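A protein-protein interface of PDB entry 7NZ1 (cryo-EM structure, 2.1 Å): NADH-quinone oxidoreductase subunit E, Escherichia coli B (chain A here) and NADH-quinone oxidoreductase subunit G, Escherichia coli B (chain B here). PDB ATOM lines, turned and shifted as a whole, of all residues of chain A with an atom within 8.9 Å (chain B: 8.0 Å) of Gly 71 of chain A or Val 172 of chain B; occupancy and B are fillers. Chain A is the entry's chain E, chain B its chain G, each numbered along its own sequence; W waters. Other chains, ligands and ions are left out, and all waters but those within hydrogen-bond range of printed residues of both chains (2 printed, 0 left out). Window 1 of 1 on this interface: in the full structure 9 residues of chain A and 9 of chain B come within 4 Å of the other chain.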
ATOM      1  N   SER A  36      38.332  24.087 -13.559  1.00  0.00           N
ATOM      2  CA  SER A  36      37.851  22.778 -13.121  1.00  0.00           C
ATOM      3  C   SER A  36      38.778  21.630 -13.514  1.00  0.00           C
ATOM      4  O   SER A  36      38.963  20.701 -12.722  1.00  0.00           O
ATOM      5  CB  SER A  36      36.435  22.545 -13.642  1.00  0.00           C
ATOM      6  OG  SER A  36      36.158  21.166 -13.789  1.00  0.00           O
ATOM      7  N   ILE A  37      39.329  21.650 -14.737  1.00  0.00           N
ATOM      8  CA  ILE A  37      40.255  20.598 -15.173  1.00  0.00           C
ATOM      9  C   ILE A  37      41.518  20.588 -14.312  1.00  0.00           C
ATOM     10  O   ILE A  37      41.947  19.534 -13.828  1.00  0.00           O
ATOM     11  CB  ILE A  37      40.591  20.747 -16.672  1.00  0.00           C
ATOM     12  CG1 ILE A  37      39.499  20.134 -17.541  1.00  0.00           C
ATOM     13  CG2 ILE A  37      41.910  20.070 -17.040  1.00  0.00           C
ATOM     14  CD1 ILE A  37      39.235  20.906 -18.825  1.00  0.00           C
ATOM     15  N   LEU A  40      40.921  19.315 -10.741  1.00  0.00           N
ATOM     16  CA  LEU A  40      40.874  17.858 -10.693  1.00  0.00           C
ATOM     17  C   LEU A  40      42.272  17.252 -10.777  1.00  0.00           C
ATOM     18  O   LEU A  40      42.565  16.272 -10.086  1.00  0.00           O
ATOM     19  CB  LEU A  40      39.987  17.334 -11.818  1.00  0.00           C
ATOM     20  CG  LEU A  40      38.492  17.593 -11.632  1.00  0.00           C
ATOM     21  CD1 LEU A  40      37.791  17.536 -12.967  1.00  0.00           C
ATOM     22  CD2 LEU A  40      37.871  16.616 -10.669  1.00  0.00           C
ATOM     23  N   ILE A  55      34.516  15.608  -5.603  1.00  0.00           N
ATOM     24  CA  ILE A  55      33.675  16.213  -6.630  1.00  0.00           C
ATOM     25  C   ILE A  55      32.863  17.362  -6.043  1.00  0.00           C
ATOM     26  O   ILE A  55      32.825  18.464  -6.600  1.00  0.00           O
ATOM     27  CB  ILE A  55      32.781  15.141  -7.278  1.00  0.00           C
ATOM     28  CG1 ILE A  55      33.657  14.081  -7.952  1.00  0.00           C
ATOM     29  CG2 ILE A  55      31.826  15.762  -8.276  1.00  0.00           C
ATOM     30  CD1 ILE A  55      34.503  14.616  -9.085  1.00  0.00           C
ATOM     31  N   ILE A  64      30.428  26.109  -9.074  1.00  0.00           N
ATOM     32  CA  ILE A  64      29.692  25.451 -10.152  1.00  0.00           C
ATOM     33  C   ILE A  64      29.068  24.197  -9.554  1.00  0.00           C
ATOM     34  O   ILE A  64      29.515  23.734  -8.491  1.00  0.00           O
ATOM     35  CB  ILE A  64      30.605  25.153 -11.367  1.00  0.00           C
ATOM     36  CG1 ILE A  64      31.910  24.495 -10.935  1.00  0.00           C
ATOM     37  CG2 ILE A  64      30.871  26.418 -12.169  1.00  0.00           C
ATOM     38  CD1 ILE A  64      32.594  23.790 -12.056  1.00  0.00           C
ATOM     39  N   PRO A  65      27.986  23.668 -10.144  1.00  0.00           N
ATOM     40  CA  PRO A  65      27.371  22.456  -9.587  1.00  0.00           C
ATOM     41  C   PRO A  65      28.257  21.226  -9.713  1.00  0.00           C
ATOM     42  O   PRO A  65      29.156  21.145 -10.553  1.00  0.00           O
ATOM     43  CB  PRO A  65      26.089  22.282 -10.411  1.00  0.00           C
ATOM     44  CG  PRO A  65      25.814  23.590 -10.979  1.00  0.00           C
ATOM     45  CD  PRO A  65      27.120  24.266 -11.180  1.00  0.00           C
ATOM     46  N   ALA A  66      27.986  20.263  -8.831  1.00  0.00           N
ATOM     47  CA  ALA A  66      28.778  19.041  -8.768  1.00  0.00           C
ATOM     48  C   ALA A  66      28.572  18.154  -9.988  1.00  0.00           C
ATOM     49  O   ALA A  66      29.476  17.396 -10.351  1.00  0.00           O
ATOM     50  CB  ALA A  66      28.437  18.267  -7.499  1.00  0.00           C
ATOM     51  N   SER A  67      27.394  18.222 -10.619  1.00  0.00           N
ATOM     52  CA  SER A  67      27.158  17.456 -11.838  1.00  0.00           C
ATOM     53  C   SER A  67      27.987  17.982 -13.005  1.00  0.00           C
ATOM     54  O   SER A  67      28.297  17.225 -13.930  1.00  0.00           O
ATOM     55  CB  SER A  67      25.671  17.474 -12.193  1.00  0.00           C
ATOM     56  OG  SER A  67      25.233  18.790 -12.479  1.00  0.00           O
ATOM     57  N   ASP A  68      28.368  19.259 -12.971  1.00  0.00           N
ATOM     58  CA  ASP A  68      29.282  19.789 -13.976  1.00  0.00           C
ATOM     59  C   ASP A  68      30.702  19.277 -13.748  1.00  0.00           C
ATOM     60  O   ASP A  68      31.418  18.981 -14.712  1.00  0.00           O
ATOM     61  CB  ASP A  68      29.250  21.315 -13.963  1.00  0.00           C
ATOM     62  CG  ASP A  68      27.950  21.880 -14.511  1.00  0.00           C
ATOM     63  OD1 ASP A  68      26.963  21.123 -14.628  1.00  0.00           O
ATOM     64  OD2 ASP A  68      27.909  23.091 -14.814  1.00  0.00           O
ATOM     65  N   VAL A  69      31.139  19.223 -12.484  1.00  0.00           N
ATOM     66  CA  VAL A  69      32.466  18.712 -12.142  1.00  0.00           C
ATOM     67  C   VAL A  69      32.579  17.225 -12.472  1.00  0.00           C
ATOM     68  O   VAL A  69      33.581  16.775 -13.044  1.00  0.00           O
ATOM     69  CB  VAL A  69      32.769  18.995 -10.655  1.00  0.00           C
ATOM     70  CG1 VAL A  69      34.060  18.307 -10.202  1.00  0.00           C
ATOM     71  CG2 VAL A  69      32.849  20.479 -10.414  1.00  0.00           C
ATOM     72  N   GLU A  70      31.552  16.445 -12.125  1.00  0.00           N
ATOM     73  CA  GLU A  70      31.533  15.011 -12.413  1.00  0.00           C
ATOM     74  C   GLU A  70      31.463  14.740 -13.915  1.00  0.00           C
ATOM     75  O   GLU A  70      32.019  13.745 -14.394  1.00  0.00           O
ATOM     76  CB  GLU A  70      30.370  14.345 -11.670  1.00  0.00           C
ATOM     77  CG  GLU A  70      30.251  12.794 -11.720  1.00  0.00           C
ATOM     78  CD  GLU A  70      31.425  11.962 -11.143  1.00  0.00           C
ATOM     79  OE1 GLU A  70      32.441  12.487 -10.646  1.00  0.00           O
ATOM     80  OE2 GLU A  70      31.302  10.724 -11.173  1.00  0.00           O
ATOM     81  N   GLY A  71      30.730  15.580 -14.652  1.00  0.00           N
ATOM     82  CA  GLY A  71      30.705  15.483 -16.106  1.00  0.00           C
ATOM     83  C   GLY A  71      32.073  15.655 -16.745  1.00  0.00           C
ATOM     84  O   GLY A  71      32.429  14.920 -17.668  1.00  0.00           O
ATOM     85  N   VAL A  72      32.836  16.651 -16.285  1.00  0.00           N
ATOM     86  CA  VAL A  72      34.190  16.878 -16.787  1.00  0.00           C
ATOM     87  C   VAL A  72      35.115  15.707 -16.444  1.00  0.00           C
ATOM     88  O   VAL A  72      35.865  15.224 -17.301  1.00  0.00           O
ATOM     89  CB  VAL A  72      34.725  18.217 -16.243  1.00  0.00           C
ATOM     90  CG1 VAL A  72      36.241  18.263 -16.270  1.00  0.00           C
ATOM     91  CG2 VAL A  72      34.124  19.372 -17.023  1.00  0.00           C
ATOM     92  N   ALA A  73      35.021  15.186 -15.213  1.00  0.00           N
ATOM     93  CA  ALA A  73      35.988  14.196 -14.738  1.00  0.00           C
ATOM     94  C   ALA A  73      35.796  12.848 -15.422  1.00  0.00           C
ATOM     95  O   ALA A  73      36.774  12.157 -15.724  1.00  0.00           O
ATOM     96  CB  ALA A  73      35.882  14.039 -13.220  1.00  0.00           C
ATOM     97  N   THR A  74      34.548  12.474 -15.697  1.00  0.00           N
ATOM     98  CA  THR A  74      34.297  11.233 -16.418  1.00  0.00           C
ATOM     99  C   THR A  74      34.628  11.363 -17.902  1.00  0.00           C
ATOM    100  O   THR A  74      34.957  10.364 -18.544  1.00  0.00           O
ATOM    101  CB  THR A  74      32.847  10.782 -16.215  1.00  0.00           C
ATOM    102  OG1 THR A  74      31.949  11.834 -16.583  1.00  0.00           O
ATOM    103  CG2 THR A  74      32.606  10.391 -14.770  1.00  0.00           C
ATOM    104  N   PHE A  75      34.505  12.568 -18.466  1.00  0.00           N
ATOM    105  CA  PHE A  75      34.814  12.788 -19.878  1.00  0.00           C
ATOM    106  C   PHE A  75      36.303  12.618 -20.184  1.00  0.00           C
ATOM    107  O   PHE A  75      36.665  11.987 -21.182  1.00  0.00           O
ATOM    108  CB  PHE A  75      34.332  14.177 -20.307  1.00  0.00           C
ATOM    109  CG  PHE A  75      34.557  14.472 -21.757  1.00  0.00           C
ATOM    110  CD1 PHE A  75      33.710  13.944 -22.721  1.00  0.00           C
ATOM    111  CD2 PHE A  75      35.599  15.296 -22.160  1.00  0.00           C
ATOM    112  CE1 PHE A  75      33.921  14.199 -24.059  1.00  0.00           C
ATOM    113  CE2 PHE A  75      35.809  15.563 -23.493  1.00  0.00           C
ATOM    114  CZ  PHE A  75      34.961  15.022 -24.446  1.00  0.00           C
ATOM    115  N   TYR A  76      37.176  13.172 -19.351  1.00  0.00           N
ATOM    116  CA  TYR A  76      38.609  13.177 -19.629  1.00  0.00           C
ATOM    117  C   TYR A  76      39.273  11.899 -19.125  1.00  0.00           C
ATOM    118  O   TYR A  76      39.094  11.513 -17.966  1.00  0.00           O
ATOM    119  CB  TYR A  76      39.248  14.420 -19.022  1.00  0.00           C
ATOM    120  CG  TYR A  76      38.837  15.690 -19.741  1.00  0.00           C
ATOM    121  CD1 TYR A  76      39.222  15.923 -21.057  1.00  0.00           C
ATOM    122  CD2 TYR A  76      38.026  16.633 -19.122  1.00  0.00           C
ATOM    123  CE1 TYR A  76      38.834  17.071 -21.725  1.00  0.00           C
ATOM    124  CE2 TYR A  76      37.624  17.777 -19.779  1.00  0.00           C
ATOM    125  CZ  TYR A  76      38.031  17.994 -21.080  1.00  0.00           C
ATOM    126  OH  TYR A  76      37.638  19.136 -21.730  1.00  0.00           O
ATOM    127  N   SER A  77      40.030  11.249 -20.019  1.00  0.00           N
ATOM    128  CA  SER A  77      40.619   9.936 -19.747  1.00  0.00           C
ATOM    129  C   SER A  77      41.667   9.969 -18.637  1.00  0.00           C
ATOM    130  O   SER A  77      41.733   9.045 -17.822  1.00  0.00           O
ATOM    131  CB  SER A  77      41.228   9.361 -21.028  1.00  0.00           C
ATOM    132  OG  SER A  77      42.177  10.243 -21.594  1.00  0.00           O
ATOM    133  N   ILE A  79      42.075  12.091 -16.055  1.00  0.00           N
ATOM    134  CA  ILE A  79      41.478  12.273 -14.735  1.00  0.00           C
ATOM    135  C   ILE A  79      40.849  10.953 -14.299  1.00  0.00           C
ATOM    136  O   ILE A  79      39.970  10.413 -14.977  1.00  0.00           O
ATOM    137  CB  ILE A  79      40.455  13.416 -14.756  1.00  0.00           C
ATOM    138  CG1 ILE A  79      41.166  14.746 -15.003  1.00  0.00           C
ATOM    139  CG2 ILE A  79      39.670  13.467 -13.464  1.00  0.00           C
ATOM    140  CD1 ILE A  79      40.302  15.782 -15.636  1.00  0.00           C
ATOM    141  N   ARG A  81      38.817   8.369 -11.736  1.00  0.00           N
ATOM    142  CA  ARG A  81      37.750   8.290 -10.744  1.00  0.00           C
ATOM    143  C   ARG A  81      37.683   6.915 -10.089  1.00  0.00           C
ATOM    144  O   ARG A  81      36.683   6.591  -9.443  1.00  0.00           O
ATOM    145  CB  ARG A  81      36.403   8.651 -11.381  1.00  0.00           C
ATOM    146  CG  ARG A  81      36.253  10.132 -11.736  1.00  0.00           C
ATOM    147  CD  ARG A  81      35.970  11.043 -10.540  1.00  0.00           C
ATOM    148  NE  ARG A  81      34.674  10.779  -9.920  1.00  0.00           N
ATOM    149  CZ  ARG A  81      34.491  10.070  -8.814  1.00  0.00           C
ATOM    150  NH1 ARG A  81      35.508   9.548  -8.151  1.00  0.00           N
ATOM    151  NH2 ARG A  81      33.253   9.865  -8.372  1.00  0.00           N
ATOM    152  N   ALA B 153      20.583   9.210 -26.372  1.00  0.00           N
ATOM    153  CA  ALA B 153      21.552  10.317 -26.278  1.00  0.00           C
ATOM    154  C   ALA B 153      21.124  11.533 -27.103  1.00  0.00           C
ATOM    155  O   ALA B 153      21.899  12.094 -27.872  1.00  0.00           O
ATOM    156  CB  ALA B 153      22.970   9.864 -26.649  1.00  0.00           C
ATOM    157  N   TYR B 155      20.054  14.326 -25.644  1.00  0.00           N
ATOM    158  CA  TYR B 155      20.445  15.432 -24.763  1.00  0.00           C
ATOM    159  C   TYR B 155      19.288  16.351 -24.394  1.00  0.00           C
ATOM    160  O   TYR B 155      19.537  17.439 -23.880  1.00  0.00           O
ATOM    161  CB  TYR B 155      21.595  16.290 -25.335  1.00  0.00           C
ATOM    162  CG  TYR B 155      22.926  15.575 -25.445  1.00  0.00           C
ATOM    163  CD1 TYR B 155      23.161  14.657 -26.462  1.00  0.00           C
ATOM    164  CD2 TYR B 155      23.948  15.821 -24.534  1.00  0.00           C
ATOM    165  CE1 TYR B 155      24.364  13.995 -26.569  1.00  0.00           C
ATOM    166  CE2 TYR B 155      25.161  15.158 -24.630  1.00  0.00           C
ATOM    167  CZ  TYR B 155      25.360  14.245 -25.649  1.00  0.00           C
ATOM    168  OH  TYR B 155      26.555  13.584 -25.766  1.00  0.00           O
ATOM    169  N   CYS B 157      17.078  15.921 -21.990  1.00  0.00           N
ATOM    170  CA  CYS B 157      16.882  15.958 -20.545  1.00  0.00           C
ATOM    171  C   CYS B 157      17.790  16.980 -19.877  1.00  0.00           C
ATOM    172  O   CYS B 157      17.335  17.746 -19.027  1.00  0.00           O
ATOM    173  CB  CYS B 157      17.123  14.572 -19.957  1.00  0.00           C
ATOM    174  SG  CYS B 157      18.693  13.850 -20.443  1.00  0.00           S
ATOM    175  N   VAL B 158      19.064  17.030 -20.271  1.00  0.00           N
ATOM    176  CA  VAL B 158      19.999  17.961 -19.650  1.00  0.00           C
ATOM    177  C   VAL B 158      19.748  19.386 -20.127  1.00  0.00           C
ATOM    178  O   VAL B 158      19.939  20.343 -19.371  1.00  0.00           O
ATOM    179  CB  VAL B 158      21.456  17.511 -19.876  1.00  0.00           C
ATOM    180  CG1 VAL B 158      21.766  16.333 -18.973  1.00  0.00           C
ATOM    181  CG2 VAL B 158      21.703  17.129 -21.319  1.00  0.00           C
ATOM    182  N   LYS B 162      19.075  21.740 -16.953  1.00  0.00           N
ATOM    183  CA  LYS B 162      20.041  22.780 -16.603  1.00  0.00           C
ATOM    184  C   LYS B 162      19.742  24.108 -17.285  1.00  0.00           C
ATOM    185  O   LYS B 162      19.743  25.150 -16.630  1.00  0.00           O
ATOM    186  CB  LYS B 162      21.489  22.410 -16.957  1.00  0.00           C
ATOM    187  CG  LYS B 162      21.972  21.002 -16.819  1.00  0.00           C
ATOM    188  CD  LYS B 162      23.411  20.986 -17.370  1.00  0.00           C
ATOM    189  CE  LYS B 162      24.164  19.714 -17.065  1.00  0.00           C
ATOM    190  NZ  LYS B 162      24.579  19.655 -15.636  1.00  0.00           N
ATOM    191  N   ASP B 169      21.281  19.240 -10.461  1.00  0.00           N
ATOM    192  CA  ASP B 169      21.721  17.902 -10.082  1.00  0.00           C
ATOM    193  C   ASP B 169      21.546  16.852 -11.181  1.00  0.00           C
ATOM    194  O   ASP B 169      21.614  15.656 -10.893  1.00  0.00           O
ATOM    195  CB  ASP B 169      21.002  17.453  -8.812  1.00  0.00           C
ATOM    196  CG  ASP B 169      19.502  17.453  -8.960  1.00  0.00           C
ATOM    197  OD1 ASP B 169      18.932  18.505  -9.307  1.00  0.00           O
ATOM    198  OD2 ASP B 169      18.893  16.393  -8.732  1.00  0.00           O
ATOM    199  N   LEU B 170      21.349  17.259 -12.431  1.00  0.00           N
ATOM    200  CA  LEU B 170      21.339  16.330 -13.554  1.00  0.00           C
ATOM    201  C   LEU B 170      22.396  16.757 -14.560  1.00  0.00           C
ATOM    202  O   LEU B 170      22.476  17.935 -14.912  1.00  0.00           O
ATOM    203  CB  LEU B 170      19.964  16.268 -14.223  1.00  0.00           C
ATOM    204  CG  LEU B 170      19.624  15.029 -15.052  1.00  0.00           C
ATOM    205  CD1 LEU B 170      19.069  13.919 -14.187  1.00  0.00           C
ATOM    206  CD2 LEU B 170      18.649  15.384 -16.164  1.00  0.00           C
ATOM    207  N   GLY B 171      23.202  15.804 -15.018  1.00  0.00           N
ATOM    208  CA  GLY B 171      24.196  16.081 -16.031  1.00  0.00           C
ATOM    209  C   GLY B 171      24.470  14.873 -16.898  1.00  0.00           C
ATOM    210  O   GLY B 171      23.882  13.806 -16.718  1.00  0.00           O
ATOM    211  N   VAL B 172      25.367  15.061 -17.863  1.00  0.00           N
ATOM    212  CA  VAL B 172      25.829  13.993 -18.744  1.00  0.00           C
ATOM    213  C   VAL B 172      27.238  13.580 -18.323  1.00  0.00           C
ATOM    214  O   VAL B 172      28.078  14.424 -17.986  1.00  0.00           O
ATOM    215  CB  VAL B 172      25.741  14.437 -20.225  1.00  0.00           C
ATOM    216  CG1 VAL B 172      26.473  15.752 -20.478  1.00  0.00           C
ATOM    217  CG2 VAL B 172      26.215  13.351 -21.182  1.00  0.00           C
ATOM    218  N   TYR B 173      27.492  12.272 -18.306  1.00  0.00           N
ATOM    219  CA  TYR B 173      28.764  11.723 -17.858  1.00  0.00           C
ATOM    220  C   TYR B 173      29.319  10.802 -18.931  1.00  0.00           C
ATOM    221  O   TYR B 173      28.581  10.268 -19.758  1.00  0.00           O
ATOM    222  CB  TYR B 173      28.587  10.960 -16.538  1.00  0.00           C
ATOM    223  CG  TYR B 173      27.713  11.731 -15.595  1.00  0.00           C
ATOM    224  CD1 TYR B 173      28.147  12.930 -15.039  1.00  0.00           C
ATOM    225  CD2 TYR B 173      26.411  11.317 -15.341  1.00  0.00           C
ATOM    226  CE1 TYR B 173      27.327  13.663 -14.211  1.00  0.00           C
ATOM    227  CE2 TYR B 173      25.584  12.043 -14.516  1.00  0.00           C
ATOM    228  CZ  TYR B 173      26.046  13.215 -13.956  1.00  0.00           C
ATOM    229  OH  TYR B 173      25.217  13.933 -13.137  1.00  0.00           O
ATOM    230  N   GLY B 174      30.629  10.609 -18.900  1.00  0.00           N
ATOM    231  CA  GLY B 174      31.278   9.686 -19.807  1.00  0.00           C
ATOM    232  C   GLY B 174      31.649  10.332 -21.127  1.00  0.00           C
ATOM    233  O   GLY B 174      31.716  11.553 -21.268  1.00  0.00           O
ATOM    234  N   ALA B 175      31.864   9.476 -22.121  1.00  0.00           N
ATOM    235  CA  ALA B 175      32.257   9.897 -23.462  1.00  0.00           C
ATOM    236  C   ALA B 175      31.921   8.773 -24.428  1.00  0.00           C
ATOM    237  O   ALA B 175      31.584   7.662 -24.013  1.00  0.00           O
ATOM    238  CB  ALA B 175      33.742  10.254 -23.539  1.00  0.00           C
ATOM    239  N   ASN B 178      29.423   5.543 -24.471  1.00  0.00           N
ATOM    240  CA  ASN B 178      29.157   5.208 -23.079  1.00  0.00           C
ATOM    241  C   ASN B 178      28.555   6.384 -22.295  1.00  0.00           C
ATOM    242  O   ASN B 178      28.665   6.418 -21.067  1.00  0.00           O
ATOM    243  CB  ASN B 178      30.437   4.685 -22.419  1.00  0.00           C
ATOM    244  CG  ASN B 178      30.155   3.774 -21.227  1.00  0.00           C
ATOM    245  OD1 ASN B 178      29.446   2.782 -21.353  1.00  0.00           O
ATOM    246  ND2 ASN B 178      30.721   4.105 -20.076  1.00  0.00           N
ATOM    247  N   VAL B 179      27.998   7.384 -22.992  1.00  0.00           N
ATOM    248  CA  VAL B 179      27.429   8.566 -22.338  1.00  0.00           C
ATOM    249  C   VAL B 179      26.255   8.189 -21.436  1.00  0.00           C
ATOM    250  O   VAL B 179      25.391   7.385 -21.803  1.00  0.00           O
ATOM    251  CB  VAL B 179      27.023   9.629 -23.375  1.00  0.00           C
ATOM    252  CG1 VAL B 179      28.243  10.367 -23.879  1.00  0.00           C
ATOM    253  CG2 VAL B 179      26.263   9.020 -24.536  1.00  0.00           C
ATOM    254  N   TYR B 180      26.243   8.755 -20.230  1.00  0.00           N
ATOM    255  CA  TYR B 180      25.280   8.425 -19.188  1.00  0.00           C
ATOM    256  C   TYR B 180      24.597   9.700 -18.718  1.00  0.00           C
ATOM    257  O   TYR B 180      25.265  10.674 -18.362  1.00  0.00           O
ATOM    258  CB  TYR B 180      25.978   7.709 -18.016  1.00  0.00           C
ATOM    259  CG  TYR B 180      25.083   7.052 -16.983  1.00  0.00           C
ATOM    260  CD1 TYR B 180      24.489   7.787 -15.955  1.00  0.00           C
ATOM    261  CD2 TYR B 180      24.839   5.686 -17.033  1.00  0.00           C
ATOM    262  CE1 TYR B 180      23.676   7.174 -15.013  1.00  0.00           C
ATOM    263  CE2 TYR B 180      24.036   5.067 -16.100  1.00  0.00           C
ATOM    264  CZ  TYR B 180      23.454   5.812 -15.097  1.00  0.00           C
ATOM    265  OH  TYR B 180      22.657   5.180 -14.180  1.00  0.00           O
ATOM    266  N   PHE B 181      23.272   9.693 -18.728  1.00  0.00           N
ATOM    267  CA  PHE B 181      22.473  10.832 -18.302  1.00  0.00           C
ATOM    268  C   PHE B 181      21.849  10.515 -16.949  1.00  0.00           C
ATOM    269  O   PHE B 181      21.153   9.506 -16.804  1.00  0.00           O
ATOM    270  CB  PHE B 181      21.412  11.170 -19.349  1.00  0.00           C
ATOM    271  CG  PHE B 181      21.985  11.665 -20.653  1.00  0.00           C
ATOM    272  CD1 PHE B 181      22.356  10.771 -21.651  1.00  0.00           C
ATOM    273  CD2 PHE B 181      22.157  13.018 -20.877  1.00  0.00           C
ATOM    274  CE1 PHE B 181      22.897  11.221 -22.840  1.00  0.00           C
ATOM    275  CE2 PHE B 181      22.684  13.477 -22.069  1.00  0.00           C
ATOM    276  CZ  PHE B 181      23.055  12.582 -23.052  1.00  0.00           C
ATOM    277  N   GLY B 182      22.103  11.368 -15.962  1.00  0.00           N
ATOM    278  CA  GLY B 182      21.556  11.139 -14.638  1.00  0.00           C
ATOM    279  C   GLY B 182      22.157  12.087 -13.619  1.00  0.00           C
ATOM    280  O   GLY B 182      22.612  13.177 -13.956  1.00  0.00           O
ATOM    281  N   ARG B 183      22.132  11.651 -12.380  1.00  0.00           N
ATOM    282  CA  ARG B 183      22.666  12.345 -11.221  1.00  0.00           C
ATOM    283  C   ARG B 183      24.084  11.864 -10.934  1.00  0.00           C
ATOM    284  O   ARG B 183      24.475  10.788 -11.389  1.00  0.00           O
ATOM    285  CB  ARG B 183      21.762  12.101 -10.015  1.00  0.00           C
ATOM    286  CG  ARG B 183      20.387  12.690 -10.094  1.00  0.00           C
ATOM    287  CD  ARG B 183      19.650  12.525  -8.773  1.00  0.00           C
ATOM    288  NE  ARG B 183      19.713  13.715  -7.932  1.00  0.00           N
ATOM    289  CZ  ARG B 183      20.506  13.854  -6.878  1.00  0.00           C
ATOM    290  NH1 ARG B 183      21.321  12.887  -6.494  1.00  0.00           N
ATOM    291  NH2 ARG B 183      20.482  14.994  -6.195  1.00  0.00           N
ATOM    292  N   PRO B 184      24.899  12.651 -10.208  1.00  0.00           N
ATOM    293  CA  PRO B 184      26.230  12.146  -9.807  1.00  0.00           C
ATOM    294  C   PRO B 184      26.173  10.941  -8.881  1.00  0.00           C
ATOM    295  O   PRO B 184      27.073  10.095  -8.919  1.00  0.00           O
ATOM    296  CB  PRO B 184      26.871  13.355  -9.111  1.00  0.00           C
ATOM    297  CG  PRO B 184      26.143  14.526  -9.630  1.00  0.00           C
ATOM    298  CD  PRO B 184      24.753  14.088  -9.896  1.00  0.00           C
HETATM  299  O   HOH W   1      27.677  17.163 -17.177  1.00  0.00           O
HETATM  300  O   HOH W   2      23.827  21.474 -14.017  1.00  0.00           O
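The side-chain amino group (NZ) of Lys 162 of chain B sits at hydrogen-bond distance from the side-chain hydroxyl (OG) of Ser 67 of chain A, at 3.3 Å. The side-chain amino group (NZ) of Lys 162 of chain B is in salt-bridge range of the side-chain carboxylate (OD1) of Asp 68 of chain A (3.0 Å). OG1 of Thr 74 of chain A lies within hydrogen-bond range of N of Gly 174 of chain B (2.9 Å).
The backbone carbonyl oxygen (O) of Glu 70 of chain A sits at hydrogen-bond distance from the side-chain hydroxyl (OG1) of Thr 74 of chain A, at 2.9 Å. The side-chain carboxylate (OE1) of Glu 70 of chain A lies within salt-bridge range of the guanidinium group (NE) of Arg 81 of chain A, at 2.9 Å. O of Gly 71 of chain A lies within hydrogen-bond range of OG1 of Thr 74 of chain A (3.3 Å). The side-chain amino group of Lys 162 of chain B sits at hydrogen-bond distance from the backbone carbonyl oxygen of Leu 170 of chain B (2.8 Å). N of Tyr 173 of chain B sits at hydrogen-bond distance from O of Tyr 180 of chain B (2.7 Å). The side-chain hydroxyl of Tyr 173 of chain B lies within hydrogen-bond range of the backbone carbonyl oxygen of Gly 182 of chain B (2.8 Å).
OG of Ser 67 of chain A touches O of Leu 170 of chain B (3.8 Å). Ser 67 of chain A touches Tyr 173 of chain B (CB to OH, 3.7 Å). Pro 184 of chain B touches Ser 67 of chain A (CG to CA, 3.8 Å). Glu 70 of chain A touches Tyr 173 of chain B (CG to CD1, 3.9 Å). Val 172 of chain B touches Gly 71 of chain A (O to CA, 3.4 Å). Gly 71 of chain A touches Tyr 173 of chain B. Thr 74 of chain A touches Tyr 173 of chain B (OG1 to CA, 3.4 Å). Phe 75 of chain A touches Gly 174 of chain B (CD1 to O, 3.4 Å). Phe 75 of chain A touches Ala 175 of chain B.
Gly 71 of chain A touches just these residues of chain B: Val 172 and Tyr 173. Of the printed residues of chain A, Lys 162 of chain B touches Ser 67 (3.3 Å) and Asp 68 (3.0 Å). Of the printed residues of chain A, Pro 184 of chain B touches Ser 67. The nearest residue of chain A that does not touch Val 172 of chain B is Thr 74 of chain A (4.9 Å).
Printed residues of chain A that touch a printed residue of chain B: Ser 67, Asp 68, Glu 70, Gly 71, Thr 74 and Phe 75. Hydrophobic or aromatic side chains of chain B that line the printed part of chain A: Tyr 173, Ala 175 and Pro 184. Among the printed residues, Asp or Glu carboxylates within 4 Å of a Lys or Arg side-chain nitrogen of the other chain: Asp 68 of chain A with Lys 162 of chain B (3.0 Å).
Water W2 lies within hydrogen-bond range of the side-chain amino group (NZ) of Lys 162 of chain B (2.5 Å), the side-chain carboxylate (OD1) of Asp 68 of chain A (3.2 Å) and the side-chain hydroxyl (OG) of Ser 67 of chain A (3.4 Å). Water W1 bridges O of Val 172 of chain B (2.9 Å) and O of Ser 67 of chain A (3.3 Å).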
